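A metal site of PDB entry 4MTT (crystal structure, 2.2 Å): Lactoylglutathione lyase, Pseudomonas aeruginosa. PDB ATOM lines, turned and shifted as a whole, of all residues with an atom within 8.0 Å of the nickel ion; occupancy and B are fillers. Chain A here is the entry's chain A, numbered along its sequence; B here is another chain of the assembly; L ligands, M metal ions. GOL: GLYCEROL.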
ATOM      1  N   GLY A  73      25.707   2.609  22.335  1.00  0.00           N
ATOM      2  CA  GLY A  73      26.068   1.411  23.072  1.00  0.00           C
ATOM      3  C   GLY A  73      27.509   0.986  22.977  1.00  0.00           C
ATOM      4  O   GLY A  73      28.301   1.278  23.874  1.00  0.00           O
ATOM      5  N   HIS A  74      27.843   0.249  21.916  1.00  0.00           N
ATOM      6  CA  HIS A  74      29.194  -0.284  21.739  1.00  0.00           C
ATOM      7  C   HIS A  74      29.447  -0.715  20.307  1.00  0.00           C
ATOM      8  O   HIS A  74      28.547  -0.712  19.468  1.00  0.00           O
ATOM      9  CB  HIS A  74      29.386  -1.533  22.636  1.00  0.00           C
ATOM     10  CG  HIS A  74      28.301  -2.559  22.482  1.00  0.00           C
ATOM     11  ND1 HIS A  74      27.294  -2.688  23.426  1.00  0.00           N
ATOM     12  CD2 HIS A  74      28.095  -3.465  21.505  1.00  0.00           C
ATOM     13  CE1 HIS A  74      26.503  -3.659  23.001  1.00  0.00           C
ATOM     14  NE2 HIS A  74      26.944  -4.171  21.863  1.00  0.00           N
ATOM     15  N   LEU A  75      30.702  -1.104  20.048  1.00  0.00           N
ATOM     16  CA  LEU A  75      31.113  -1.702  18.806  1.00  0.00           C
ATOM     17  C   LEU A  75      31.476  -3.134  19.193  1.00  0.00           C
ATOM     18  O   LEU A  75      32.240  -3.350  20.134  1.00  0.00           O
ATOM     19  CB  LEU A  75      32.322  -0.976  18.185  1.00  0.00           C
ATOM     20  CG  LEU A  75      32.834  -1.541  16.826  1.00  0.00           C
ATOM     21  CD1 LEU A  75      31.911  -1.127  15.668  1.00  0.00           C
ATOM     22  CD2 LEU A  75      34.273  -1.058  16.534  1.00  0.00           C
ATOM     23  N   ALA A  76      30.879  -4.119  18.525  1.00  0.00           N
ATOM     24  CA  ALA A  76      31.219  -5.489  18.836  1.00  0.00           C
ATOM     25  C   ALA A  76      32.179  -6.071  17.821  1.00  0.00           C
ATOM     26  O   ALA A  76      32.011  -5.897  16.611  1.00  0.00           O
ATOM     27  CB  ALA A  76      29.971  -6.341  18.954  1.00  0.00           C
ATOM     28  N   ILE A  77      33.160  -6.807  18.314  1.00  0.00           N
ATOM     29  CA  ILE A  77      34.176  -7.431  17.462  1.00  0.00           C
ATOM     30  C   ILE A  77      34.245  -8.942  17.731  1.00  0.00           C
ATOM     31  O   ILE A  77      34.351  -9.372  18.884  1.00  0.00           O
ATOM     32  CB  ILE A  77      35.594  -6.767  17.679  1.00  0.00           C
ATOM     33  CG1 ILE A  77      35.614  -5.225  17.551  1.00  0.00           C
ATOM     34  CG2 ILE A  77      36.714  -7.502  16.851  1.00  0.00           C
ATOM     35  CD1 ILE A  77      35.260  -4.638  16.257  1.00  0.00           C
ATOM     36  N   ILE A 110      31.811 -13.600  26.203  1.00  0.00           N
ATOM     37  CA  ILE A 110      31.848 -12.174  25.937  1.00  0.00           C
ATOM     38  C   ILE A 110      32.844 -11.452  26.867  1.00  0.00           C
ATOM     39  O   ILE A 110      33.161 -11.974  27.926  1.00  0.00           O
ATOM     40  CB  ILE A 110      30.370 -11.630  25.998  1.00  0.00           C
ATOM     41  CG1 ILE A 110      29.625 -11.993  24.706  1.00  0.00           C
ATOM     42  CG2 ILE A 110      30.267 -10.100  26.257  1.00  0.00           C
ATOM     43  CD1 ILE A 110      28.105 -11.977  24.814  1.00  0.00           C
ATOM     44  N   PHE A 112      34.301  -7.031  27.794  1.00  0.00           N
ATOM     45  CA  PHE A 112      34.205  -5.611  27.485  1.00  0.00           C
ATOM     46  C   PHE A 112      35.472  -4.849  27.718  1.00  0.00           C
ATOM     47  O   PHE A 112      36.048  -4.910  28.797  1.00  0.00           O
ATOM     48  CB  PHE A 112      33.044  -4.939  28.221  1.00  0.00           C
ATOM     49  CG  PHE A 112      31.726  -5.139  27.521  1.00  0.00           C
ATOM     50  CD1 PHE A 112      30.981  -6.294  27.731  1.00  0.00           C
ATOM     51  CD2 PHE A 112      31.227  -4.175  26.654  1.00  0.00           C
ATOM     52  CE1 PHE A 112      29.762  -6.486  27.078  1.00  0.00           C
ATOM     53  CE2 PHE A 112      29.999  -4.366  26.006  1.00  0.00           C
ATOM     54  CZ  PHE A 112      29.274  -5.513  26.228  1.00  0.00           C
ATOM     55  N   GLU A 122      32.777  -4.420  22.683  1.00  0.00           N
ATOM     56  CA  GLU A 122      32.296  -5.733  23.042  1.00  0.00           C
ATOM     57  C   GLU A 122      33.058  -6.795  22.231  1.00  0.00           C
ATOM     58  O   GLU A 122      33.081  -6.764  21.003  1.00  0.00           O
ATOM     59  CB  GLU A 122      30.772  -5.797  22.770  1.00  0.00           C
ATOM     60  CG  GLU A 122      30.097  -7.120  23.082  1.00  0.00           C
ATOM     61  CD  GLU A 122      28.603  -7.038  22.882  1.00  0.00           C
ATOM     62  OE1 GLU A 122      28.145  -6.948  21.718  1.00  0.00           O
ATOM     63  OE2 GLU A 122      27.894  -6.922  23.906  1.00  0.00           O
ATOM     64  N   LEU A 123      33.651  -7.746  22.938  1.00  0.00           N
ATOM     65  CA  LEU A 123      34.359  -8.852  22.323  1.00  0.00           C
ATOM     66  C   LEU A 123      33.482 -10.079  22.390  1.00  0.00           C
ATOM     67  O   LEU A 123      32.960 -10.413  23.451  1.00  0.00           O
ATOM     68  CB  LEU A 123      35.679  -9.124  23.028  1.00  0.00           C
ATOM     69  CG  LEU A 123      36.675  -7.972  23.180  1.00  0.00           C
ATOM     70  CD1 LEU A 123      37.929  -8.477  23.836  1.00  0.00           C
ATOM     71  CD2 LEU A 123      36.995  -7.310  21.795  1.00  0.00           C
ATOM     72  N   ILE A 124      33.265 -10.716  21.247  1.00  0.00           N
ATOM     73  CA  ILE A 124      32.433 -11.910  21.223  1.00  0.00           C
ATOM     74  C   ILE A 124      33.295 -13.022  20.632  1.00  0.00           C
ATOM     75  O   ILE A 124      33.790 -12.888  19.519  1.00  0.00           O
ATOM     76  CB  ILE A 124      31.074 -11.701  20.508  1.00  0.00           C
ATOM     77  CG1 ILE A 124      30.296 -10.459  21.049  1.00  0.00           C
ATOM     78  CG2 ILE A 124      30.246 -12.992  20.594  1.00  0.00           C
ATOM     79  CD1 ILE A 124      28.927 -10.121  20.284  1.00  0.00           C
ATOM     80  N   LEU B   4      31.338  -7.047  14.206  1.00  0.00           N
ATOM     81  CA  LEU B   4      30.038  -7.752  14.238  1.00  0.00           C
ATOM     82  C   LEU B   4      28.856  -6.824  14.164  1.00  0.00           C
ATOM     83  O   LEU B   4      27.924  -7.069  13.415  1.00  0.00           O
ATOM     84  CB  LEU B   4      29.927  -8.611  15.493  1.00  0.00           C
ATOM     85  CG  LEU B   4      30.846  -9.833  15.555  1.00  0.00           C
ATOM     86  CD1 LEU B   4      30.845 -10.435  16.987  1.00  0.00           C
ATOM     87  CD2 LEU B   4      30.374 -10.934  14.557  1.00  0.00           C
ATOM     88  N   HIS B   5      28.864  -5.764  14.986  1.00  0.00           N
ATOM     89  CA  HIS B   5      27.762  -4.806  15.000  1.00  0.00           C
ATOM     90  C   HIS B   5      28.147  -3.524  15.747  1.00  0.00           C
ATOM     91  O   HIS B   5      29.143  -3.467  16.455  1.00  0.00           O
ATOM     92  CB  HIS B   5      26.466  -5.437  15.647  1.00  0.00           C
ATOM     93  CG  HIS B   5      26.610  -5.966  17.048  1.00  0.00           C
ATOM     94  ND1 HIS B   5      26.845  -7.318  17.296  1.00  0.00           N
ATOM     95  CD2 HIS B   5      26.467  -5.335  18.238  1.00  0.00           C
ATOM     96  CE1 HIS B   5      26.896  -7.446  18.615  1.00  0.00           C
ATOM     97  NE2 HIS B   5      26.675  -6.285  19.224  1.00  0.00           N
ATOM     98  N   SER B   6      27.313  -2.502  15.581  1.00  0.00           N
ATOM     99  CA  SER B   6      27.294  -1.252  16.330  1.00  0.00           C
ATOM    100  C   SER B   6      25.961  -1.367  17.098  1.00  0.00           C
ATOM    101  O   SER B   6      24.982  -1.875  16.534  1.00  0.00           O
ATOM    102  CB  SER B   6      27.226  -0.045  15.395  1.00  0.00           C
ATOM    103  OG  SER B   6      27.068   1.138  16.163  1.00  0.00           O
ATOM    104  N   MET B   7      25.939  -0.990  18.360  1.00  0.00           N
ATOM    105  CA  MET B   7      24.739  -1.038  19.196  1.00  0.00           C
ATOM    106  C   MET B   7      24.271   0.356  19.588  1.00  0.00           C
ATOM    107  O   MET B   7      25.079   1.184  20.019  1.00  0.00           O
ATOM    108  CB  MET B   7      24.954  -1.964  20.425  1.00  0.00           C
ATOM    109  CG  MET B   7      23.690  -2.246  21.253  1.00  0.00           C
ATOM    110  SD  MET B   7      23.073  -0.869  22.264  1.00  0.00           S
ATOM    111  CE  MET B   7      23.741  -1.271  23.860  1.00  0.00           C
ATOM    112  N   LEU B   8      22.958   0.615  19.447  1.00  0.00           N
ATOM    113  CA  LEU B   8      22.262   1.847  19.814  1.00  0.00           C
ATOM    114  C   LEU B   8      21.078   1.486  20.719  1.00  0.00           C
ATOM    115  O   LEU B   8      20.344   0.532  20.424  1.00  0.00           O
ATOM    116  CB  LEU B   8      21.735   2.605  18.580  1.00  0.00           C
ATOM    117  CG  LEU B   8      22.782   3.189  17.625  1.00  0.00           C
ATOM    118  CD1 LEU B   8      22.125   3.797  16.389  1.00  0.00           C
ATOM    119  CD2 LEU B   8      23.726   4.209  18.334  1.00  0.00           C
ATOM    120  N   ARG B  30      17.180 -10.719  13.441  1.00  0.00           N
ATOM    121  CA  ARG B  30      17.099 -11.451  14.694  1.00  0.00           C
ATOM    122  C   ARG B  30      16.522 -10.482  15.720  1.00  0.00           C
ATOM    123  O   ARG B  30      16.731  -9.267  15.640  1.00  0.00           O
ATOM    124  CB  ARG B  30      18.547 -11.924  15.036  1.00  0.00           C
ATOM    125  CG  ARG B  30      18.717 -12.825  16.222  1.00  0.00           C
ATOM    126  CD  ARG B  30      20.039 -13.594  16.175  1.00  0.00           C
ATOM    127  NE  ARG B  30      21.234 -12.748  16.049  1.00  0.00           N
ATOM    128  CZ  ARG B  30      21.995 -12.343  17.060  1.00  0.00           C
ATOM    129  NH1 ARG B  30      23.064 -11.612  16.833  1.00  0.00           N
ATOM    130  NH2 ARG B  30      21.685 -12.683  18.301  1.00  0.00           N
ATOM    131  N   LEU B  41      16.602  -7.287  22.388  1.00  0.00           N
ATOM    132  CA  LEU B  41      17.618  -7.020  21.364  1.00  0.00           C
ATOM    133  C   LEU B  41      17.012  -7.239  19.994  1.00  0.00           C
ATOM    134  O   LEU B  41      16.268  -8.203  19.822  1.00  0.00           O
ATOM    135  CB  LEU B  41      18.822  -7.959  21.517  1.00  0.00           C
ATOM    136  CG  LEU B  41      19.665  -7.819  22.793  1.00  0.00           C
ATOM    137  CD1 LEU B  41      20.913  -8.617  22.669  1.00  0.00           C
ATOM    138  CD2 LEU B  41      20.022  -6.339  23.050  1.00  0.00           C
ATOM    139  N   PHE B  43      18.351  -7.043  15.733  1.00  0.00           N
ATOM    140  CA  PHE B  43      19.460  -6.914  14.785  1.00  0.00           C
ATOM    141  C   PHE B  43      18.900  -6.643  13.403  1.00  0.00           C
ATOM    142  O   PHE B  43      18.183  -7.481  12.851  1.00  0.00           O
ATOM    143  CB  PHE B  43      20.330  -8.183  14.757  1.00  0.00           C
ATOM    144  CG  PHE B  43      20.947  -8.457  16.096  1.00  0.00           C
ATOM    145  CD1 PHE B  43      20.221  -9.094  17.110  1.00  0.00           C
ATOM    146  CD2 PHE B  43      22.254  -8.057  16.371  1.00  0.00           C
ATOM    147  CE1 PHE B  43      20.793  -9.329  18.363  1.00  0.00           C
ATOM    148  CE2 PHE B  43      22.829  -8.314  17.616  1.00  0.00           C
ATOM    149  CZ  PHE B  43      22.088  -8.937  18.621  1.00  0.00           C
ATOM    150  N   GLU B  56      22.660  -3.365  16.002  1.00  0.00           N
ATOM    151  CA  GLU B  56      21.997  -3.916  17.176  1.00  0.00           C
ATOM    152  C   GLU B  56      21.236  -2.814  17.882  1.00  0.00           C
ATOM    153  O   GLU B  56      21.792  -1.725  18.138  1.00  0.00           O
ATOM    154  CB  GLU B  56      23.006  -4.588  18.094  1.00  0.00           C
ATOM    155  CG  GLU B  56      22.392  -5.157  19.357  1.00  0.00           C
ATOM    156  CD  GLU B  56      23.386  -5.829  20.268  1.00  0.00           C
ATOM    157  OE1 GLU B  56      24.363  -5.163  20.690  1.00  0.00           O
ATOM    158  OE2 GLU B  56      23.244  -7.048  20.483  1.00  0.00           O
ATOM    159  N   LEU B  57      19.941  -3.067  18.099  1.00  0.00           N
ATOM    160  CA  LEU B  57      19.034  -2.145  18.783  1.00  0.00           C
ATOM    161  C   LEU B  57      18.676  -2.716  20.139  1.00  0.00           C
ATOM    162  O   LEU B  57      18.212  -3.850  20.224  1.00  0.00           O
ATOM    163  CB  LEU B  57      17.755  -1.847  17.941  1.00  0.00           C
ATOM    164  CG  LEU B  57      17.970  -1.165  16.552  1.00  0.00           C
ATOM    165  CD1 LEU B  57      16.674  -1.098  15.782  1.00  0.00           C
ATOM    166  CD2 LEU B  57      18.623   0.196  16.666  1.00  0.00           C
ATOM    167  N   THR B  58      18.930  -1.951  21.194  1.00  0.00           N
ATOM    168  CA  THR B  58      18.611  -2.379  22.559  1.00  0.00           C
ATOM    169  C   THR B  58      17.433  -1.583  23.116  1.00  0.00           C
ATOM    170  O   THR B  58      17.473  -0.357  23.222  1.00  0.00           O
ATOM    171  CB  THR B  58      19.870  -2.321  23.472  1.00  0.00           C
ATOM    172  OG1 THR B  58      20.883  -3.121  22.875  1.00  0.00           O
ATOM    173  CG2 THR B  58      19.612  -2.869  24.872  1.00  0.00           C
HETATM  174  C1  GOL L   1      25.057  -7.964  23.655  1.00  0.00           C
HETATM  175  O1  GOL L   1      25.308  -6.603  23.332  1.00  0.00           O
HETATM  176  C2  GOL L   1      24.778  -8.732  22.382  1.00  0.00           C
HETATM  177  O2  GOL L   1      25.643  -8.278  21.354  1.00  0.00           O
HETATM  178  C3  GOL L   1      24.833 -10.236  22.508  1.00  0.00           C
HETATM  179  O3  GOL L   1      26.163 -10.702  22.612  1.00  0.00           O
HETATM  180 NI    NI M   1      26.249  -6.093  21.216  1.00  0.00          NI
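The backbone carbonyl oxygen (O) of His 5 of chain B lies within hydrogen-bond range of the backbone NH (N) of Ala 76, 2.8 Å away. The backbone NH of Glu 122 lies within hydrogen-bond range of the backbone carbonyl oxygen of Leu 75, at 2.8 Å. The backbone NH of Ile 77 is in hydrogen-bond range of the backbone carbonyl oxygen of Glu 122 (2.7 Å). N of Met 7 of chain B is in hydrogen-bond range of O of His 74. O of Ser 6 of chain B lies within hydrogen-bond range of N of Glu 56 of chain B (2.8 Å). The backbone carbonyl oxygen of Glu 56 of chain B sits at hydrogen-bond distance from the backbone NH of Leu 8 of chain B (2.9 Å).
The nickel ion is bound by NE2 of His 5 of chain B (2.0 Å), OE1 of Glu 122 (2.1 Å), NE2 of His 74 (2.1 Å), OE1 of Glu 56 of chain B (2.2 Å), O2 of the ligand (2.3 Å) and O1 of the ligand (2.4 Å). The nickel ion has six donor atoms within binding distance.
Four residues have an atom within 4 Å of the nickel ion: His 74, Glu 122, His 5 of chain B and Glu 56 of chain B.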
